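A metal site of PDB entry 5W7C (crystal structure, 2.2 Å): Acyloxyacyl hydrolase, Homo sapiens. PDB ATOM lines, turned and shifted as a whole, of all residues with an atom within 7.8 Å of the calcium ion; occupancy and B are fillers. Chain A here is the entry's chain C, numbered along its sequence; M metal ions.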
ATOM      1  N   CYS A  54     -10.185   1.017   1.266  1.00  0.00           N
ATOM      2  CA  CYS A  54     -11.028   1.170   2.441  1.00  0.00           C
ATOM      3  C   CYS A  54     -10.387   0.604   3.702  1.00  0.00           C
ATOM      4  O   CYS A  54     -10.854   0.918   4.800  1.00  0.00           O
ATOM      5  CB  CYS A  54     -12.387   0.496   2.200  1.00  0.00           C
ATOM      6  SG  CYS A  54     -12.310  -1.221   1.612  1.00  0.00           S
ATOM      7  N   ARG A  65     -11.909  -6.940  -5.504  1.00  0.00           N
ATOM      8  CA  ARG A  65     -11.843  -8.281  -4.957  1.00  0.00           C
ATOM      9  C   ARG A  65     -13.242  -8.886  -4.864  1.00  0.00           C
ATOM     10  O   ARG A  65     -14.233  -8.187  -4.642  1.00  0.00           O
ATOM     11  CB  ARG A  65     -11.186  -8.262  -3.583  1.00  0.00           C
ATOM     12  CG  ARG A  65     -10.847  -9.641  -3.028  1.00  0.00           C
ATOM     13  CD  ARG A  65     -10.040  -9.525  -1.749  1.00  0.00           C
ATOM     14  NE  ARG A  65      -9.902 -10.817  -1.068  1.00  0.00           N
ATOM     15  CZ  ARG A  65      -8.824 -11.582  -1.111  1.00  0.00           C
ATOM     16  NH1 ARG A  65      -7.752 -11.222  -1.805  1.00  0.00           N
ATOM     17  NH2 ARG A  65      -8.808 -12.742  -0.450  1.00  0.00           N
ATOM     18  N   ARG A  66     -13.319 -10.206  -5.032  1.00  0.00           N
ATOM     19  CA  ARG A  66     -14.572 -10.891  -4.803  1.00  0.00           C
ATOM     20  C   ARG A  66     -14.896 -10.864  -3.310  1.00  0.00           C
ATOM     21  O   ARG A  66     -13.985 -10.968  -2.483  1.00  0.00           O
ATOM     22  CB  ARG A  66     -14.516 -12.337  -5.301  1.00  0.00           C
ATOM     23  CG  ARG A  66     -14.229 -12.482  -6.795  1.00  0.00           C
ATOM     24  CD  ARG A  66     -14.736 -13.806  -7.344  1.00  0.00           C
ATOM     25  NE  ARG A  66     -16.080 -13.678  -7.928  1.00  0.00           N
ATOM     26  CZ  ARG A  66     -16.340 -13.586  -9.226  1.00  0.00           C
ATOM     27  NH1 ARG A  66     -15.363 -13.615 -10.120  1.00  0.00           N
ATOM     28  NH2 ARG A  66     -17.599 -13.460  -9.634  1.00  0.00           N
ATOM     29  N   PRO A  67     -16.168 -10.726  -2.930  1.00  0.00           N
ATOM     30  CA  PRO A  67     -16.485 -10.559  -1.507  1.00  0.00           C
ATOM     31  C   PRO A  67     -15.951 -11.716  -0.668  1.00  0.00           C
ATOM     32  O   PRO A  67     -15.988 -12.878  -1.072  1.00  0.00           O
ATOM     33  CB  PRO A  67     -18.018 -10.525  -1.492  1.00  0.00           C
ATOM     34  CG  PRO A  67     -18.418 -10.164  -2.878  1.00  0.00           C
ATOM     35  CD  PRO A  67     -17.373 -10.748  -3.770  1.00  0.00           C
ATOM     36  N   ASN A  68     -15.435 -11.365   0.510  1.00  0.00           N
ATOM     37  CA  ASN A  68     -14.942 -12.355   1.467  1.00  0.00           C
ATOM     38  C   ASN A  68     -16.127 -12.833   2.297  1.00  0.00           C
ATOM     39  O   ASN A  68     -16.522 -12.185   3.268  1.00  0.00           O
ATOM     40  CB  ASN A  68     -13.851 -11.756   2.346  1.00  0.00           C
ATOM     41  CG  ASN A  68     -13.343 -12.734   3.377  1.00  0.00           C
ATOM     42  OD1 ASN A  68     -13.345 -13.946   3.165  1.00  0.00           O
ATOM     43  ND2 ASN A  68     -12.901 -12.210   4.525  1.00  0.00           N
ATOM     44  N   TRP A  70     -19.213 -12.819   1.501  1.00  0.00           N
ATOM     45  CA  TRP A  70     -20.313 -11.871   1.293  1.00  0.00           C
ATOM     46  C   TRP A  70     -20.211 -10.647   2.193  1.00  0.00           C
ATOM     47  O   TRP A  70     -21.231  -9.997   2.474  1.00  0.00           O
ATOM     48  CB  TRP A  70     -21.666 -12.564   1.499  1.00  0.00           C
ATOM     49  CG  TRP A  70     -21.873 -13.673   0.529  1.00  0.00           C
ATOM     50  CD1 TRP A  70     -21.997 -15.010   0.819  1.00  0.00           C
ATOM     51  CD2 TRP A  70     -21.962 -13.566  -0.892  1.00  0.00           C
ATOM     52  NE1 TRP A  70     -22.169 -15.729  -0.340  1.00  0.00           N
ATOM     53  CE2 TRP A  70     -22.146 -14.862  -1.408  1.00  0.00           C
ATOM     54  CE3 TRP A  70     -21.909 -12.492  -1.792  1.00  0.00           C
ATOM     55  CZ2 TRP A  70     -22.279 -15.125  -2.772  1.00  0.00           C
ATOM     56  CZ3 TRP A  70     -22.037 -12.748  -3.144  1.00  0.00           C
ATOM     57  CH2 TRP A  70     -22.229 -14.054  -3.624  1.00  0.00           C
ATOM     58  N   ASP A  71     -19.004 -10.296   2.640  1.00  0.00           N
ATOM     59  CA  ASP A  71     -18.771  -9.065   3.386  1.00  0.00           C
ATOM     60  C   ASP A  71     -19.709  -8.958   4.593  1.00  0.00           C
ATOM     61  O   ASP A  71     -20.361  -7.928   4.808  1.00  0.00           O
ATOM     62  CB  ASP A  71     -18.903  -7.845   2.474  1.00  0.00           C
ATOM     63  CG  ASP A  71     -17.790  -7.761   1.448  1.00  0.00           C
ATOM     64  OD1 ASP A  71     -17.037  -8.742   1.293  1.00  0.00           O
ATOM     65  OD2 ASP A  71     -17.663  -6.702   0.790  1.00  0.00           O
ATOM     66  N   GLN A  74     -16.881  -7.228   7.086  1.00  0.00           N
ATOM     67  CA  GLN A  74     -16.041  -6.192   6.508  1.00  0.00           C
ATOM     68  C   GLN A  74     -16.395  -6.014   5.038  1.00  0.00           C
ATOM     69  O   GLN A  74     -16.742  -6.982   4.347  1.00  0.00           O
ATOM     70  CB  GLN A  74     -14.552  -6.524   6.647  1.00  0.00           C
ATOM     71  CG  GLN A  74     -13.768  -5.539   7.498  1.00  0.00           C
ATOM     72  CD  GLN A  74     -12.314  -5.423   7.091  1.00  0.00           C
ATOM     73  OE1 GLN A  74     -11.859  -4.368   6.668  1.00  0.00           O
ATOM     74  NE2 GLN A  74     -11.575  -6.521   7.223  1.00  0.00           N
ATOM     75  N   ASP A  75     -16.293  -4.776   4.572  1.00  0.00           N
ATOM     76  CA  ASP A  75     -16.398  -4.464   3.155  1.00  0.00           C
ATOM     77  C   ASP A  75     -15.050  -4.785   2.514  1.00  0.00           C
ATOM     78  O   ASP A  75     -14.127  -3.968   2.533  1.00  0.00           O
ATOM     79  CB  ASP A  75     -16.777  -3.001   2.952  1.00  0.00           C
ATOM     80  CG  ASP A  75     -16.886  -2.615   1.493  1.00  0.00           C
ATOM     81  OD1 ASP A  75     -16.714  -1.421   1.173  1.00  0.00           O
ATOM     82  OD2 ASP A  75     -17.151  -3.518   0.668  1.00  0.00           O
ATOM     83  N   SER A  76     -14.939  -5.988   1.951  1.00  0.00           N
ATOM     84  CA  SER A  76     -13.656  -6.481   1.467  1.00  0.00           C
ATOM     85  C   SER A  76     -13.275  -5.941   0.098  1.00  0.00           C
ATOM     86  O   SER A  76     -12.112  -6.101  -0.311  1.00  0.00           O
ATOM     87  CB  SER A  76     -13.665  -8.016   1.426  1.00  0.00           C
ATOM     88  OG  SER A  76     -14.545  -8.496   0.424  1.00  0.00           O
ATOM     89  N   ASN A  77     -14.200  -5.309  -0.639  1.00  0.00           N
ATOM     90  CA  ASN A  77     -13.893  -4.758  -1.958  1.00  0.00           C
ATOM     91  C   ASN A  77     -14.167  -3.256  -2.044  1.00  0.00           C
ATOM     92  O   ASN A  77     -14.261  -2.719  -3.154  1.00  0.00           O
ATOM     93  CB  ASN A  77     -14.665  -5.508  -3.044  1.00  0.00           C
ATOM     94  CG  ASN A  77     -16.136  -5.635  -2.729  1.00  0.00           C
ATOM     95  OD1 ASN A  77     -16.687  -4.863  -1.943  1.00  0.00           O
ATOM     96  ND2 ASN A  77     -16.785  -6.613  -3.351  1.00  0.00           N
ATOM     97  N   CYS A  78     -14.310  -2.587  -0.908  1.00  0.00           N
ATOM     98  CA  CYS A  78     -14.355  -1.123  -0.848  1.00  0.00           C
ATOM     99  C   CYS A  78     -15.462  -0.530  -1.705  1.00  0.00           C
ATOM    100  O   CYS A  78     -15.393   0.657  -2.066  1.00  0.00           O
ATOM    101  CB  CYS A  78     -13.012  -0.525  -1.271  1.00  0.00           C
ATOM    102  SG  CYS A  78     -11.596  -1.096  -0.291  1.00  0.00           S
ATOM    103  N   ASN A  79     -16.500  -1.298  -2.040  1.00  0.00           N
ATOM    104  CA  ASN A  79     -17.623  -0.769  -2.799  1.00  0.00           C
ATOM    105  C   ASN A  79     -18.724  -0.204  -1.908  1.00  0.00           C
ATOM    106  O   ASN A  79     -19.775   0.182  -2.409  1.00  0.00           O
ATOM    107  CB  ASN A  79     -18.197  -1.836  -3.731  1.00  0.00           C
ATOM    108  CG  ASN A  79     -18.785  -3.008  -2.972  1.00  0.00           C
ATOM    109  OD1 ASN A  79     -18.860  -3.007  -1.742  1.00  0.00           O
ATOM    110  ND2 ASN A  79     -19.219  -4.031  -3.708  1.00  0.00           N
ATOM    111  N   GLY A  80     -18.491  -0.135  -0.599  1.00  0.00           N
ATOM    112  CA  GLY A  80     -19.450   0.420   0.328  1.00  0.00           C
ATOM    113  C   GLY A  80     -20.601  -0.503   0.668  1.00  0.00           C
ATOM    114  O   GLY A  80     -21.431  -0.138   1.508  1.00  0.00           O
ATOM    115  N   ILE A  81     -20.674  -1.685   0.064  1.00  0.00           N
ATOM    116  CA  ILE A  81     -21.754  -2.631   0.302  1.00  0.00           C
ATOM    117  C   ILE A  81     -21.213  -3.729   1.225  1.00  0.00           C
ATOM    118  O   ILE A  81     -20.235  -4.400   0.878  1.00  0.00           O
ATOM    119  CB  ILE A  81     -22.282  -3.225  -1.014  1.00  0.00           C
ATOM    120  CG1 ILE A  81     -22.764  -2.115  -1.943  1.00  0.00           C
ATOM    121  CG2 ILE A  81     -23.402  -4.234  -0.740  1.00  0.00           C
ATOM    122  CD1 ILE A  81     -23.022  -2.563  -3.371  1.00  0.00           C
ATOM    123  N   TRP A  82     -21.837  -3.895   2.371  1.00  0.00           N
ATOM    124  CA  TRP A  82     -21.455  -4.951   3.308  1.00  0.00           C
ATOM    125  C   TRP A  82     -22.554  -5.063   4.355  1.00  0.00           C
ATOM    126  O   TRP A  82     -23.623  -4.451   4.233  1.00  0.00           O
ATOM    127  CB  TRP A  82     -20.082  -4.652   3.938  1.00  0.00           C
ATOM    128  CG  TRP A  82     -20.083  -3.519   4.909  1.00  0.00           C
ATOM    129  CD1 TRP A  82     -20.271  -2.198   4.625  1.00  0.00           C
ATOM    130  CD2 TRP A  82     -19.878  -3.595   6.325  1.00  0.00           C
ATOM    131  NE1 TRP A  82     -20.197  -1.452   5.774  1.00  0.00           N
ATOM    132  CE2 TRP A  82     -19.961  -2.280   6.825  1.00  0.00           C
ATOM    133  CE3 TRP A  82     -19.637  -4.654   7.208  1.00  0.00           C
ATOM    134  CZ2 TRP A  82     -19.803  -1.993   8.182  1.00  0.00           C
ATOM    135  CZ3 TRP A  82     -19.485  -4.360   8.554  1.00  0.00           C
ATOM    136  CH2 TRP A  82     -19.566  -3.051   9.031  1.00  0.00           C
ATOM    137  N   GLY A  83     -22.294  -5.852   5.400  1.00  0.00           N
ATOM    138  CA  GLY A  83     -23.267  -6.052   6.457  1.00  0.00           C
ATOM    139  C   GLY A  83     -24.365  -7.022   6.067  1.00  0.00           C
ATOM    140  O   GLY A  83     -24.351  -7.649   4.996  1.00  0.00           O
ATOM    141  N   TYR A  92     -25.985  -8.115   2.498  1.00  0.00           N
ATOM    142  CA  TYR A  92     -26.352  -7.111   1.498  1.00  0.00           C
ATOM    143  C   TYR A  92     -25.620  -7.345   0.182  1.00  0.00           C
ATOM    144  O   TYR A  92     -26.204  -7.189  -0.890  1.00  0.00           O
ATOM    145  CB  TYR A  92     -26.052  -5.706   2.040  1.00  0.00           C
ATOM    146  CG  TYR A  92     -27.150  -5.124   2.903  1.00  0.00           C
ATOM    147  CD1 TYR A  92     -26.923  -4.802   4.236  1.00  0.00           C
ATOM    148  CD2 TYR A  92     -28.421  -4.907   2.385  1.00  0.00           C
ATOM    149  CE1 TYR A  92     -27.926  -4.264   5.016  1.00  0.00           C
ATOM    150  CE2 TYR A  92     -29.432  -4.384   3.160  1.00  0.00           C
ATOM    151  CZ  TYR A  92     -29.174  -4.058   4.477  1.00  0.00           C
ATOM    152  OH  TYR A  92     -30.185  -3.534   5.252  1.00  0.00           O
ATOM    153  N   GLU A  93     -24.338  -7.713   0.244  1.00  0.00           N
ATOM    154  CA  GLU A  93     -23.606  -7.937  -0.991  1.00  0.00           C
ATOM    155  C   GLU A  93     -24.160  -9.126  -1.762  1.00  0.00           C
ATOM    156  O   GLU A  93     -24.148  -9.126  -3.002  1.00  0.00           O
ATOM    157  CB  GLU A  93     -22.112  -8.150  -0.690  1.00  0.00           C
ATOM    158  CG  GLU A  93     -21.232  -8.325  -1.928  1.00  0.00           C
ATOM    159  CD  GLU A  93     -20.367  -7.124  -2.240  1.00  0.00           C
ATOM    160  OE1 GLU A  93     -19.807  -7.072  -3.361  1.00  0.00           O
ATOM    161  OE2 GLU A  93     -20.222  -6.220  -1.383  1.00  0.00           O
ATOM    162  N   CYS A  97     -25.515  -7.759  -5.132  1.00  0.00           N
ATOM    163  CA  CYS A  97     -24.433  -7.881  -6.100  1.00  0.00           C
ATOM    164  C   CYS A  97     -24.296  -9.271  -6.709  1.00  0.00           C
ATOM    165  O   CYS A  97     -23.839  -9.369  -7.854  1.00  0.00           O
ATOM    166  CB  CYS A  97     -23.096  -7.494  -5.457  1.00  0.00           C
ATOM    167  SG  CYS A  97     -23.046  -5.773  -4.871  1.00  0.00           S
ATOM    168  N   CYS A 177     -22.333  -1.940  -7.704  1.00  0.00           N
ATOM    169  CA  CYS A 177     -21.369  -2.778  -7.016  1.00  0.00           C
ATOM    170  C   CYS A 177     -19.938  -2.526  -7.477  1.00  0.00           C
ATOM    171  O   CYS A 177     -18.994  -2.924  -6.801  1.00  0.00           O
ATOM    172  CB  CYS A 177     -21.735  -4.254  -7.181  1.00  0.00           C
ATOM    173  SG  CYS A 177     -23.391  -4.685  -6.562  1.00  0.00           S
ATOM    174  N   TYR A 210     -12.628  -9.898  -9.211  1.00  0.00           N
ATOM    175  CA  TYR A 210     -13.602  -9.892 -10.285  1.00  0.00           C
ATOM    176  C   TYR A 210     -12.910  -9.722 -11.637  1.00  0.00           C
ATOM    177  O   TYR A 210     -11.773  -9.249 -11.717  1.00  0.00           O
ATOM    178  CB  TYR A 210     -14.599  -8.751 -10.101  1.00  0.00           C
ATOM    179  CG  TYR A 210     -15.682  -9.009  -9.086  1.00  0.00           C
ATOM    180  CD1 TYR A 210     -16.649  -9.983  -9.298  1.00  0.00           C
ATOM    181  CD2 TYR A 210     -15.760  -8.257  -7.914  1.00  0.00           C
ATOM    182  CE1 TYR A 210     -17.647 -10.214  -8.380  1.00  0.00           C
ATOM    183  CE2 TYR A 210     -16.753  -8.481  -6.983  1.00  0.00           C
ATOM    184  CZ  TYR A 210     -17.696  -9.466  -7.217  1.00  0.00           C
ATOM    185  OH  TYR A 210     -18.691  -9.689  -6.304  1.00  0.00           O
ATOM    186  N   PHE A 417     -27.052   2.352   1.293  1.00  0.00           N
ATOM    187  CA  PHE A 417     -25.664   2.758   1.448  1.00  0.00           C
ATOM    188  C   PHE A 417     -25.365   4.166   0.937  1.00  0.00           C
ATOM    189  O   PHE A 417     -24.249   4.655   1.163  1.00  0.00           O
ATOM    190  CB  PHE A 417     -24.756   1.752   0.727  1.00  0.00           C
ATOM    191  CG  PHE A 417     -24.866   0.353   1.269  1.00  0.00           C
ATOM    192  CD1 PHE A 417     -24.206  -0.008   2.433  1.00  0.00           C
ATOM    193  CD2 PHE A 417     -25.624  -0.599   0.614  1.00  0.00           C
ATOM    194  CE1 PHE A 417     -24.316  -1.291   2.939  1.00  0.00           C
ATOM    195  CE2 PHE A 417     -25.729  -1.889   1.114  1.00  0.00           C
ATOM    196  CZ  PHE A 417     -25.071  -2.235   2.279  1.00  0.00           C
HETATM  197 CA    CA M   1     -18.464  -4.977  -0.458  1.00  0.00          CA
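OD1 of Asp 75 lies close to N of Cys 78, 3.4 Å away.
N of Gly 80 lies within hydrogen-bond range of OD1 of Asp 75 (2.8 Å).
OD1 of Asp 71 sits at hydrogen-bond distance from OG of Ser 76.
N of Gly 83 is in hydrogen-bond range of O of Asp 71 (2.9 Å).
The side-chain amide nitrogen (ND2) of Asn 77 lies close to the backbone carbonyl oxygen (O) of Arg 65.
The side-chain amide nitrogen of Asn 79 lies within hydrogen-bond range of the backbone carbonyl oxygen of Cys 177 (3.3 Å).
SG of Cys 78 is disulfide-bonded to SG of Cys 54 (2.0 Å).
The side-chain sulfur (SG) of Cys 97 is disulfide-bonded to the side-chain sulfur (SG) of Cys 177 (2.0 Å).
OD2 of Asp 75 is bound to the calcium ion (2.3 Å).
The calcium ion is bound by the side-chain carboxylate (OD2) of Asp 71 (2.3 Å).
The backbone carbonyl oxygen (O) of Ile 81 binds the calcium ion (2.3 Å).
OD1 of Asn 77 binds the calcium ion (2.3 Å).
OE2 of Glu 93 binds the calcium ion, at 2.3 Å.
The calcium ion is bound by OD1 of Asn 79 (2.4 Å).
The calcium ion has six donor atoms within binding distance.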
